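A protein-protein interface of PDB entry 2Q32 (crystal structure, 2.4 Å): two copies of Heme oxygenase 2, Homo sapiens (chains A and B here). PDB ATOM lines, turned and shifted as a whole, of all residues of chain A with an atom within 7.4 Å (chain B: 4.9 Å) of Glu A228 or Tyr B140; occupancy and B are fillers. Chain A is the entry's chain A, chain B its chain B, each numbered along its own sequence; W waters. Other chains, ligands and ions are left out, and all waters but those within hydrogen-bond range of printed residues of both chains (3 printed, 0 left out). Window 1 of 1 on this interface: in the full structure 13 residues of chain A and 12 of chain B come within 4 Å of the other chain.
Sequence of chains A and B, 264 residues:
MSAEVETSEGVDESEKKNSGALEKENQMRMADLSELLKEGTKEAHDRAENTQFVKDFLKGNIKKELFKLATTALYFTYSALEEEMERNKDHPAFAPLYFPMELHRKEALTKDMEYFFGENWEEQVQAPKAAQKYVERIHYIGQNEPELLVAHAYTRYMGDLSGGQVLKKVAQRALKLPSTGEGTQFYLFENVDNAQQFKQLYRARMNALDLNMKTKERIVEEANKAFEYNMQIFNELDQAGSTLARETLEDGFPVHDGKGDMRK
The side-chain amide nitrogen (ND2) of Asn A224 sits close to the side-chain amide oxygen (OD1) of Asn B144.
The side-chain carboxylate of Glu A228 is in salt-bridge range of the guanidinium group of Arg B137, 3.0 Å away.
NH1 of Arg A47 lies within salt-bridge range of OE1 of Glu A228.
The side-chain carboxylate (OE2) of Glu A221 is in salt-bridge range of the side-chain amino group (NZ) of Lys A225.
The side-chain hydroxyl (OH) of Tyr B140 lies within hydrogen-bond range of the side-chain carboxylate (OE2) of Glu B145, at 2.6 Å.
The side-chain carboxylate of Glu A228 sits at hydrogen-bond distance from the side-chain amide nitrogen of Gln A232, at 2.8 Å.
The side-chain amide nitrogen (ND2) of Asn A235 is in hydrogen-bond range of the side-chain amide oxygen (OE1) of Gln A232 (3.3 Å).
O of His B139 lies close to NE2 of Gln B143 (3.4 Å).
Among the printed residues, pairs that only touch across the chains: Arg A47 with Glu B136, Arg A47 with His B139, Arg A47 with Tyr B140, Arg A47 with Gln B143, Asn A224 with Tyr B140, Lys A225 with Tyr B140, Glu A228 with Tyr B140, Met A231 with Glu B136 and Gln A232 with Arg B137.
Glu A228 touches just these residues of chain B: Arg B137 and Tyr B140.
Of the printed residues of chain A, Tyr B140 touches Arg A47, Asn A224, Lys A225 and Glu A228.
Of the printed residues of chain B, Met A231 touches Glu B136.
Of the printed residues of chain B, Gln A232 touches Arg B137.
Glu B145 touches none of the printed residues of chain A.
The nearest residue of chain B that does not touch Glu A228 is Glu B136 (4.7 Å).
The nearest printed residue of chain A that does not touch Tyr B140 is Glu A221 (5.4 Å).
No position is printed for both chains.
Of the 11 pairs that touch across the chains among the printed residues, none has its exchanged pair printed and touching as well.
Water W3 lies within hydrogen-bond range of NH1 of Arg A47 (2.5 Å), OE1 of Glu A228 (2.6 Å) and O of Glu B136 (3.1 Å).
Water W1 lies within hydrogen-bond range of OE1 of Gln B143 (2.6 Å), NH2 of Arg A47 (2.9 Å) and ND2 of Asn B144 (2.9 Å).
Water W2 lies within hydrogen-bond range of the side-chain carboxylate (OE2) of Glu A221 (2.9 Å), the side-chain amino group (NZ) of Lys A225 (3.0 Å) and the backbone carbonyl oxygen (O) of Asn B144 (3.3 Å).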
ATOM      1  N   ALA A  44       8.040 -12.855 -14.067  1.00  0.00           N
ATOM      2  CA  ALA A  44       8.155 -12.613 -12.642  1.00  0.00           C
ATOM      3  C   ALA A  44       7.219 -13.523 -11.819  1.00  0.00           C
ATOM      4  O   ALA A  44       7.628 -14.100 -10.802  1.00  0.00           O
ATOM      5  CB  ALA A  44       7.901 -11.129 -12.335  1.00  0.00           C
ATOM      6  N   ARG A  47       8.570 -17.029 -11.774  1.00  0.00           N
ATOM      7  CA  ARG A  47       9.693 -17.219 -10.854  1.00  0.00           C
ATOM      8  C   ARG A  47       9.256 -17.339  -9.398  1.00  0.00           C
ATOM      9  O   ARG A  47       9.845 -18.104  -8.644  1.00  0.00           O
ATOM     10  CB  ARG A  47      10.760 -16.128 -11.030  1.00  0.00           C
ATOM     11  CG  ARG A  47      11.753 -16.462 -12.128  1.00  0.00           C
ATOM     12  CD  ARG A  47      12.887 -15.460 -12.236  1.00  0.00           C
ATOM     13  NE  ARG A  47      12.503 -14.341 -13.100  1.00  0.00           N
ATOM     14  CZ  ARG A  47      12.108 -13.161 -12.644  1.00  0.00           C
ATOM     15  NH1 ARG A  47      12.073 -12.951 -11.327  1.00  0.00           N
ATOM     16  NH2 ARG A  47      11.757 -12.194 -13.497  1.00  0.00           N
ATOM     17  N   ALA A  48       8.224 -16.589  -9.020  1.00  0.00           N
ATOM     18  CA  ALA A  48       7.693 -16.628  -7.658  1.00  0.00           C
ATOM     19  C   ALA A  48       6.933 -17.930  -7.344  1.00  0.00           C
ATOM     20  O   ALA A  48       7.049 -18.480  -6.248  1.00  0.00           O
ATOM     21  CB  ALA A  48       6.815 -15.407  -7.408  1.00  0.00           C
ATOM     22  N   TYR A 134      11.359  -3.136   0.973  1.00  0.00           N
ATOM     23  CA  TYR A 134      10.054  -3.031   0.324  1.00  0.00           C
ATOM     24  C   TYR A 134       9.251  -1.880   0.930  1.00  0.00           C
ATOM     25  O   TYR A 134       8.656  -1.084   0.206  1.00  0.00           O
ATOM     26  CB  TYR A 134       9.253  -4.343   0.370  1.00  0.00           C
ATOM     27  CG  TYR A 134       7.849  -4.157  -0.186  1.00  0.00           C
ATOM     28  CD1 TYR A 134       7.588  -4.321  -1.549  1.00  0.00           C
ATOM     29  CD2 TYR A 134       6.784  -3.749   0.647  1.00  0.00           C
ATOM     30  CE1 TYR A 134       6.311  -4.128  -2.070  1.00  0.00           C
ATOM     31  CE2 TYR A 134       5.494  -3.523   0.128  1.00  0.00           C
ATOM     32  CZ  TYR A 134       5.269  -3.724  -1.229  1.00  0.00           C
ATOM     33  OH  TYR A 134       3.999  -3.523  -1.752  1.00  0.00           O
ATOM     34  N   GLU A 221       5.859  -1.962 -14.963  1.00  0.00           N
ATOM     35  CA  GLU A 221       7.246  -1.898 -14.522  1.00  0.00           C
ATOM     36  C   GLU A 221       7.369  -1.999 -12.996  1.00  0.00           C
ATOM     37  O   GLU A 221       8.246  -2.688 -12.466  1.00  0.00           O
ATOM     38  CB  GLU A 221       7.842  -0.577 -15.003  1.00  0.00           C
ATOM     39  CG  GLU A 221       9.279  -0.647 -15.424  1.00  0.00           C
ATOM     40  CD  GLU A 221       9.913   0.734 -15.621  1.00  0.00           C
ATOM     41  OE1 GLU A 221       9.175   1.737 -15.790  1.00  0.00           O
ATOM     42  OE2 GLU A 221      11.159   0.811 -15.590  1.00  0.00           O
ATOM     43  N   GLU A 222       6.486  -1.301 -12.299  1.00  0.00           N
ATOM     44  CA  GLU A 222       6.498  -1.256 -10.851  1.00  0.00           C
ATOM     45  C   GLU A 222       5.931  -2.564 -10.283  1.00  0.00           C
ATOM     46  O   GLU A 222       6.332  -3.000  -9.192  1.00  0.00           O
ATOM     47  CB  GLU A 222       5.712  -0.025 -10.358  1.00  0.00           C
ATOM     48  CG  GLU A 222       5.712   0.206  -8.838  1.00  0.00           C
ATOM     49  CD  GLU A 222       7.087   0.534  -8.283  1.00  0.00           C
ATOM     50  OE1 GLU A 222       7.963   0.988  -9.054  1.00  0.00           O
ATOM     51  OE2 GLU A 222       7.305   0.336  -7.076  1.00  0.00           O
ATOM     52  N   ALA A 223       5.022  -3.198 -11.031  1.00  0.00           N
ATOM     53  CA  ALA A 223       4.506  -4.528 -10.661  1.00  0.00           C
ATOM     54  C   ALA A 223       5.617  -5.572 -10.684  1.00  0.00           C
ATOM     55  O   ALA A 223       5.686  -6.416  -9.810  1.00  0.00           O
ATOM     56  CB  ALA A 223       3.371  -4.948 -11.564  1.00  0.00           C
ATOM     57  N   ASN A 224       6.485  -5.505 -11.685  1.00  0.00           N
ATOM     58  CA  ASN A 224       7.658  -6.363 -11.744  1.00  0.00           C
ATOM     59  C   ASN A 224       8.606  -6.114 -10.569  1.00  0.00           C
ATOM     60  O   ASN A 224       9.102  -7.066  -9.969  1.00  0.00           O
ATOM     61  CB  ASN A 224       8.375  -6.203 -13.082  1.00  0.00           C
ATOM     62  CG  ASN A 224       7.776  -7.071 -14.165  1.00  0.00           C
ATOM     63  OD1 ASN A 224       7.756  -8.300 -14.053  1.00  0.00           O
ATOM     64  ND2 ASN A 224       7.294  -6.439 -15.236  1.00  0.00           N
ATOM     65  N   LYS A 225       8.833  -4.844 -10.229  1.00  0.00           N
ATOM     66  CA  LYS A 225       9.640  -4.486  -9.051  1.00  0.00           C
ATOM     67  C   LYS A 225       9.035  -5.083  -7.779  1.00  0.00           C
ATOM     68  O   LYS A 225       9.755  -5.649  -6.954  1.00  0.00           O
ATOM     69  CB  LYS A 225       9.747  -2.966  -8.889  1.00  0.00           C
ATOM     70  CG  LYS A 225      10.760  -2.287  -9.782  1.00  0.00           C
ATOM     71  CD  LYS A 225      10.823  -0.784  -9.475  1.00  0.00           C
ATOM     72  CE  LYS A 225      11.941  -0.068 -10.261  1.00  0.00           C
ATOM     73  NZ  LYS A 225      11.785  -0.127 -11.759  1.00  0.00           N
ATOM     74  N   ALA A 226       7.713  -4.935  -7.644  1.00  0.00           N
ATOM     75  CA  ALA A 226       6.946  -5.484  -6.530  1.00  0.00           C
ATOM     76  C   ALA A 226       7.174  -6.992  -6.354  1.00  0.00           C
ATOM     77  O   ALA A 226       7.446  -7.435  -5.241  1.00  0.00           O
ATOM     78  CB  ALA A 226       5.443  -5.172  -6.688  1.00  0.00           C
ATOM     79  N   PHE A 227       7.072  -7.759  -7.443  1.00  0.00           N
ATOM     80  CA  PHE A 227       7.401  -9.182  -7.428  1.00  0.00           C
ATOM     81  C   PHE A 227       8.818  -9.436  -6.894  1.00  0.00           C
ATOM     82  O   PHE A 227       9.022 -10.286  -6.025  1.00  0.00           O
ATOM     83  CB  PHE A 227       7.287  -9.781  -8.828  1.00  0.00           C
ATOM     84  CG  PHE A 227       5.910 -10.269  -9.186  1.00  0.00           C
ATOM     85  CD1 PHE A 227       5.031  -9.458  -9.910  1.00  0.00           C
ATOM     86  CD2 PHE A 227       5.492 -11.560  -8.831  1.00  0.00           C
ATOM     87  CE1 PHE A 227       3.737  -9.915 -10.255  1.00  0.00           C
ATOM     88  CE2 PHE A 227       4.205 -12.028  -9.173  1.00  0.00           C
ATOM     89  CZ  PHE A 227       3.332 -11.196  -9.893  1.00  0.00           C
ATOM     90  N   GLU A 228       9.802  -8.709  -7.414  1.00  0.00           N
ATOM     91  CA  GLU A 228      11.191  -8.952  -7.022  1.00  0.00           C
ATOM     92  C   GLU A 228      11.481  -8.623  -5.554  1.00  0.00           C
ATOM     93  O   GLU A 228      12.260  -9.317  -4.927  1.00  0.00           O
ATOM     94  CB  GLU A 228      12.166  -8.225  -7.946  1.00  0.00           C
ATOM     95  CG  GLU A 228      13.637  -8.548  -7.681  1.00  0.00           C
ATOM     96  CD  GLU A 228      14.000  -9.997  -7.972  1.00  0.00           C
ATOM     97  OE1 GLU A 228      13.230 -10.712  -8.657  1.00  0.00           O
ATOM     98  OE2 GLU A 228      15.068 -10.441  -7.508  1.00  0.00           O
ATOM     99  N   TYR A 229      10.865  -7.565  -5.027  1.00  0.00           N
ATOM    100  CA  TYR A 229      10.946  -7.261  -3.597  1.00  0.00           C
ATOM    101  C   TYR A 229      10.530  -8.478  -2.769  1.00  0.00           C
ATOM    102  O   TYR A 229      11.164  -8.784  -1.757  1.00  0.00           O
ATOM    103  CB  TYR A 229      10.103  -6.032  -3.207  1.00  0.00           C
ATOM    104  CG  TYR A 229      10.779  -4.724  -3.532  1.00  0.00           C
ATOM    105  CD1 TYR A 229      10.244  -3.866  -4.498  1.00  0.00           C
ATOM    106  CD2 TYR A 229      11.968  -4.347  -2.894  1.00  0.00           C
ATOM    107  CE1 TYR A 229      10.869  -2.668  -4.815  1.00  0.00           C
ATOM    108  CE2 TYR A 229      12.599  -3.149  -3.205  1.00  0.00           C
ATOM    109  CZ  TYR A 229      12.036  -2.317  -4.169  1.00  0.00           C
ATOM    110  OH  TYR A 229      12.636  -1.126  -4.495  1.00  0.00           O
ATOM    111  N   ASN A 230       9.486  -9.174  -3.228  1.00  0.00           N
ATOM    112  CA  ASN A 230       9.069 -10.434  -2.596  1.00  0.00           C
ATOM    113  C   ASN A 230      10.046 -11.585  -2.723  1.00  0.00           C
ATOM    114  O   ASN A 230      10.311 -12.265  -1.735  1.00  0.00           O
ATOM    115  CB  ASN A 230       7.662 -10.843  -3.006  1.00  0.00           C
ATOM    116  CG  ASN A 230       6.625 -10.104  -2.223  1.00  0.00           C
ATOM    117  OD1 ASN A 230       5.448 -10.149  -2.543  1.00  0.00           O
ATOM    118  ND2 ASN A 230       7.057  -9.393  -1.184  1.00  0.00           N
ATOM    119  N   MET A 231      10.595 -11.777  -3.919  1.00  0.00           N
ATOM    120  CA  MET A 231      11.674 -12.733  -4.127  1.00  0.00           C
ATOM    121  C   MET A 231      12.799 -12.529  -3.143  1.00  0.00           C
ATOM    122  O   MET A 231      13.460 -13.489  -2.766  1.00  0.00           O
ATOM    123  CB  MET A 231      12.259 -12.615  -5.537  1.00  0.00           C
ATOM    124  CG  MET A 231      11.285 -12.940  -6.642  1.00  0.00           C
ATOM    125  SD  MET A 231      10.684 -14.646  -6.609  1.00  0.00           S
ATOM    126  CE  MET A 231      12.111 -15.520  -7.230  1.00  0.00           C
ATOM    127  N   GLN A 232      13.047 -11.281  -2.761  1.00  0.00           N
ATOM    128  CA  GLN A 232      14.168 -10.976  -1.876  1.00  0.00           C
ATOM    129  C   GLN A 232      13.787 -11.236  -0.428  1.00  0.00           C
ATOM    130  O   GLN A 232      14.612 -11.637   0.369  1.00  0.00           O
ATOM    131  CB  GLN A 232      14.687  -9.547  -2.091  1.00  0.00           C
ATOM    132  CG  GLN A 232      15.306  -9.327  -3.471  1.00  0.00           C
ATOM    133  CD  GLN A 232      16.387 -10.342  -3.806  1.00  0.00           C
ATOM    134  OE1 GLN A 232      17.285 -10.584  -3.013  1.00  0.00           O
ATOM    135  NE2 GLN A 232      16.309 -10.929  -4.993  1.00  0.00           N
ATOM    136  N   ILE A 233      12.526 -11.016  -0.098  1.00  0.00           N
ATOM    137  CA  ILE A 233      11.993 -11.444   1.186  1.00  0.00           C
ATOM    138  C   ILE A 233      12.081 -12.978   1.341  1.00  0.00           C
ATOM    139  O   ILE A 233      12.604 -13.467   2.343  1.00  0.00           O
ATOM    140  CB  ILE A 233      10.562 -10.921   1.401  1.00  0.00           C
ATOM    141  CG1 ILE A 233      10.583  -9.382   1.512  1.00  0.00           C
ATOM    142  CG2 ILE A 233       9.928 -11.593   2.652  1.00  0.00           C
ATOM    143  CD1 ILE A 233       9.205  -8.679   1.499  1.00  0.00           C
ATOM    144  N   PHE A 234      11.612 -13.723   0.337  1.00  0.00           N
ATOM    145  CA  PHE A 234      11.705 -15.191   0.337  1.00  0.00           C
ATOM    146  C   PHE A 234      13.134 -15.666   0.430  1.00  0.00           C
ATOM    147  O   PHE A 234      13.397 -16.641   1.121  1.00  0.00           O
ATOM    148  CB  PHE A 234      11.093 -15.798  -0.927  1.00  0.00           C
ATOM    149  CG  PHE A 234       9.631 -15.508  -1.107  1.00  0.00           C
ATOM    150  CD1 PHE A 234       8.813 -15.244  -0.015  1.00  0.00           C
ATOM    151  CD2 PHE A 234       9.067 -15.528  -2.377  1.00  0.00           C
ATOM    152  CE1 PHE A 234       7.439 -14.987  -0.189  1.00  0.00           C
ATOM    153  CE2 PHE A 234       7.697 -15.284  -2.565  1.00  0.00           C
ATOM    154  CZ  PHE A 234       6.881 -15.022  -1.469  1.00  0.00           C
ATOM    155  N   ASN A 235      14.034 -14.988  -0.290  1.00  0.00           N
ATOM    156  CA  ASN A 235      15.470 -15.294  -0.336  1.00  0.00           C
ATOM    157  C   ASN A 235      16.063 -15.185   1.066  1.00  0.00           C
ATOM    158  O   ASN A 235      16.750 -16.075   1.522  1.00  0.00           O
ATOM    159  CB  ASN A 235      16.164 -14.334  -1.334  1.00  0.00           C
ATOM    160  CG  ASN A 235      17.693 -14.499  -1.405  1.00  0.00           C
ATOM    161  OD1 ASN A 235      18.261 -15.513  -0.993  1.00  0.00           O
ATOM    162  ND2 ASN A 235      18.368 -13.476  -1.943  1.00  0.00           N
ATOM    163  N   GLU B 136      17.604 -16.688 -10.734  1.00  0.00           N
ATOM    164  CA  GLU B 136      16.371 -15.904 -10.629  1.00  0.00           C
ATOM    165  C   GLU B 136      16.627 -14.381 -10.600  1.00  0.00           C
ATOM    166  O   GLU B 136      15.918 -13.610 -11.270  1.00  0.00           O
ATOM    167  CB  GLU B 136      15.523 -16.370  -9.428  1.00  0.00           C
ATOM    168  CG  GLU B 136      14.904 -17.770  -9.614  1.00  0.00           C
ATOM    169  CD  GLU B 136      14.379 -18.391  -8.316  1.00  0.00           C
ATOM    170  OE1 GLU B 136      14.342 -17.711  -7.261  1.00  0.00           O
ATOM    171  OE2 GLU B 136      13.993 -19.586  -8.345  1.00  0.00           O
ATOM    172  N   ARG B 137      17.651 -13.960  -9.852  1.00  0.00           N
ATOM    173  CA  ARG B 137      17.996 -12.543  -9.751  1.00  0.00           C
ATOM    174  C   ARG B 137      18.519 -12.000 -11.077  1.00  0.00           C
ATOM    175  O   ARG B 137      18.146 -10.903 -11.510  1.00  0.00           O
ATOM    176  CB  ARG B 137      19.021 -12.307  -8.638  1.00  0.00           C
ATOM    177  CG  ARG B 137      19.423 -10.839  -8.463  1.00  0.00           C
ATOM    178  CD  ARG B 137      18.261  -9.990  -7.996  1.00  0.00           C
ATOM    179  NE  ARG B 137      18.679  -8.623  -7.698  1.00  0.00           N
ATOM    180  CZ  ARG B 137      17.878  -7.662  -7.243  1.00  0.00           C
ATOM    181  NH1 ARG B 137      16.589  -7.897  -7.017  1.00  0.00           N
ATOM    182  NH2 ARG B 137      18.376  -6.457  -6.999  1.00  0.00           N
ATOM    183  N   ILE B 138      19.388 -12.769 -11.718  1.00  0.00           N
ATOM    184  CA  ILE B 138      19.951 -12.408 -13.007  1.00  0.00           C
ATOM    185  C   ILE B 138      18.880 -12.178 -14.070  1.00  0.00           C
ATOM    186  O   ILE B 138      18.990 -11.246 -14.878  1.00  0.00           O
ATOM    187  CB  ILE B 138      20.951 -13.480 -13.486  1.00  0.00           C
ATOM    188  CG1 ILE B 138      22.248 -13.379 -12.670  1.00  0.00           C
ATOM    189  CG2 ILE B 138      21.261 -13.308 -14.976  1.00  0.00           C
ATOM    190  CD1 ILE B 138      23.141 -14.593 -12.806  1.00  0.00           C
ATOM    191  N   HIS B 139      17.859 -13.028 -14.082  1.00  0.00           N
ATOM    192  CA  HIS B 139      16.757 -12.887 -15.023  1.00  0.00           C
ATOM    193  C   HIS B 139      15.878 -11.682 -14.710  1.00  0.00           C
ATOM    194  O   HIS B 139      15.479 -10.971 -15.618  1.00  0.00           O
ATOM    195  CB  HIS B 139      15.911 -14.148 -15.067  1.00  0.00           C
ATOM    196  CG  HIS B 139      16.544 -15.276 -15.814  1.00  0.00           C
ATOM    197  ND1 HIS B 139      17.127 -15.114 -17.053  1.00  0.00           N
ATOM    198  CD2 HIS B 139      16.657 -16.593 -15.511  1.00  0.00           C
ATOM    199  CE1 HIS B 139      17.596 -16.277 -17.467  1.00  0.00           C
ATOM    200  NE2 HIS B 139      17.317 -17.194 -16.554  1.00  0.00           N
ATOM    201  N   TYR B 140      15.556 -11.460 -13.436  1.00  0.00           N
ATOM    202  CA  TYR B 140      14.874 -10.228 -13.055  1.00  0.00           C
ATOM    203  C   TYR B 140      15.620  -8.994 -13.590  1.00  0.00           C
ATOM    204  O   TYR B 140      15.029  -8.151 -14.254  1.00  0.00           O
ATOM    205  CB  TYR B 140      14.708 -10.076 -11.540  1.00  0.00           C
ATOM    206  CG  TYR B 140      14.233  -8.672 -11.238  1.00  0.00           C
ATOM    207  CD1 TYR B 140      12.885  -8.329 -11.396  1.00  0.00           C
ATOM    208  CD2 TYR B 140      15.136  -7.666 -10.881  1.00  0.00           C
ATOM    209  CE1 TYR B 140      12.444  -7.042 -11.174  1.00  0.00           C
ATOM    210  CE2 TYR B 140      14.699  -6.364 -10.660  1.00  0.00           C
ATOM    211  CZ  TYR B 140      13.350  -6.056 -10.804  1.00  0.00           C
ATOM    212  OH  TYR B 140      12.891  -4.768 -10.592  1.00  0.00           O
ATOM    213  N   ILE B 141      16.909  -8.903 -13.281  1.00  0.00           N
ATOM    214  CA  ILE B 141      17.750  -7.772 -13.655  1.00  0.00           C
ATOM    215  C   ILE B 141      17.835  -7.565 -15.173  1.00  0.00           C
ATOM    216  O   ILE B 141      17.660  -6.448 -15.654  1.00  0.00           O
ATOM    217  CB  ILE B 141      19.191  -7.896 -13.024  1.00  0.00           C
ATOM    218  CG1 ILE B 141      19.137  -7.689 -11.499  1.00  0.00           C
ATOM    219  CG2 ILE B 141      20.237  -6.963 -13.723  1.00  0.00           C
ATOM    220  CD1 ILE B 141      18.643  -6.329 -11.016  1.00  0.00           C
ATOM    221  N   GLY B 142      18.100  -8.630 -15.923  1.00  0.00           N
ATOM    222  CA  GLY B 142      18.247  -8.515 -17.376  1.00  0.00           C
ATOM    223  C   GLY B 142      16.942  -8.170 -18.084  1.00  0.00           C
ATOM    224  O   GLY B 142      16.946  -7.602 -19.187  1.00  0.00           O
ATOM    225  N   GLN B 143      15.825  -8.495 -17.439  1.00  0.00           N
ATOM    226  CA  GLN B 143      14.500  -8.262 -18.012  1.00  0.00           C
ATOM    227  C   GLN B 143      13.859  -6.943 -17.582  1.00  0.00           C
ATOM    228  O   GLN B 143      12.937  -6.462 -18.244  1.00  0.00           O
ATOM    229  CB  GLN B 143      13.562  -9.424 -17.674  1.00  0.00           C
ATOM    230  CG  GLN B 143      13.878 -10.702 -18.418  1.00  0.00           C
ATOM    231  CD  GLN B 143      13.351 -11.929 -17.722  1.00  0.00           C
ATOM    232  OE1 GLN B 143      12.337 -11.877 -17.028  1.00  0.00           O
ATOM    233  NE2 GLN B 143      14.035 -13.054 -17.909  1.00  0.00           N
ATOM    234  N   ASN B 144      14.327  -6.369 -16.477  1.00  0.00           N
ATOM    235  CA  ASN B 144      13.640  -5.230 -15.868  1.00  0.00           C
ATOM    236  C   ASN B 144      14.544  -4.082 -15.472  1.00  0.00           C
ATOM    237  O   ASN B 144      14.132  -2.927 -15.535  1.00  0.00           O
ATOM    238  CB  ASN B 144      12.833  -5.678 -14.647  1.00  0.00           C
ATOM    239  CG  ASN B 144      11.843  -6.751 -14.980  1.00  0.00           C
ATOM    240  OD1 ASN B 144      10.767  -6.464 -15.478  1.00  0.00           O
ATOM    241  ND2 ASN B 144      12.206  -8.002 -14.725  1.00  0.00           N
ATOM    242  N   GLU B 145      15.768  -4.399 -15.045  1.00  0.00           N
ATOM    243  CA  GLU B 145      16.741  -3.358 -14.696  1.00  0.00           C
ATOM    244  C   GLU B 145      18.110  -3.592 -15.348  1.00  0.00           C
ATOM    245  O   GLU B 145      19.113  -3.745 -14.644  1.00  0.00           O
ATOM    246  CB  GLU B 145      16.830  -3.212 -13.172  1.00  0.00           C
ATOM    247  CG  GLU B 145      15.453  -3.023 -12.532  1.00  0.00           C
ATOM    248  CD  GLU B 145      15.506  -2.486 -11.141  1.00  0.00           C
ATOM    249  OE1 GLU B 145      16.263  -1.530 -10.887  1.00  0.00           O
ATOM    250  OE2 GLU B 145      14.754  -3.003 -10.293  1.00  0.00           O
HETATM  251  O   HOH W   1      10.776 -10.407 -15.540  1.00  0.00           O
HETATM  252  O   HOH W   2      13.565   0.015 -14.145  1.00  0.00           O
HETATM  253  O   HOH W   3      13.598 -13.250  -9.317  1.00  0.00           O
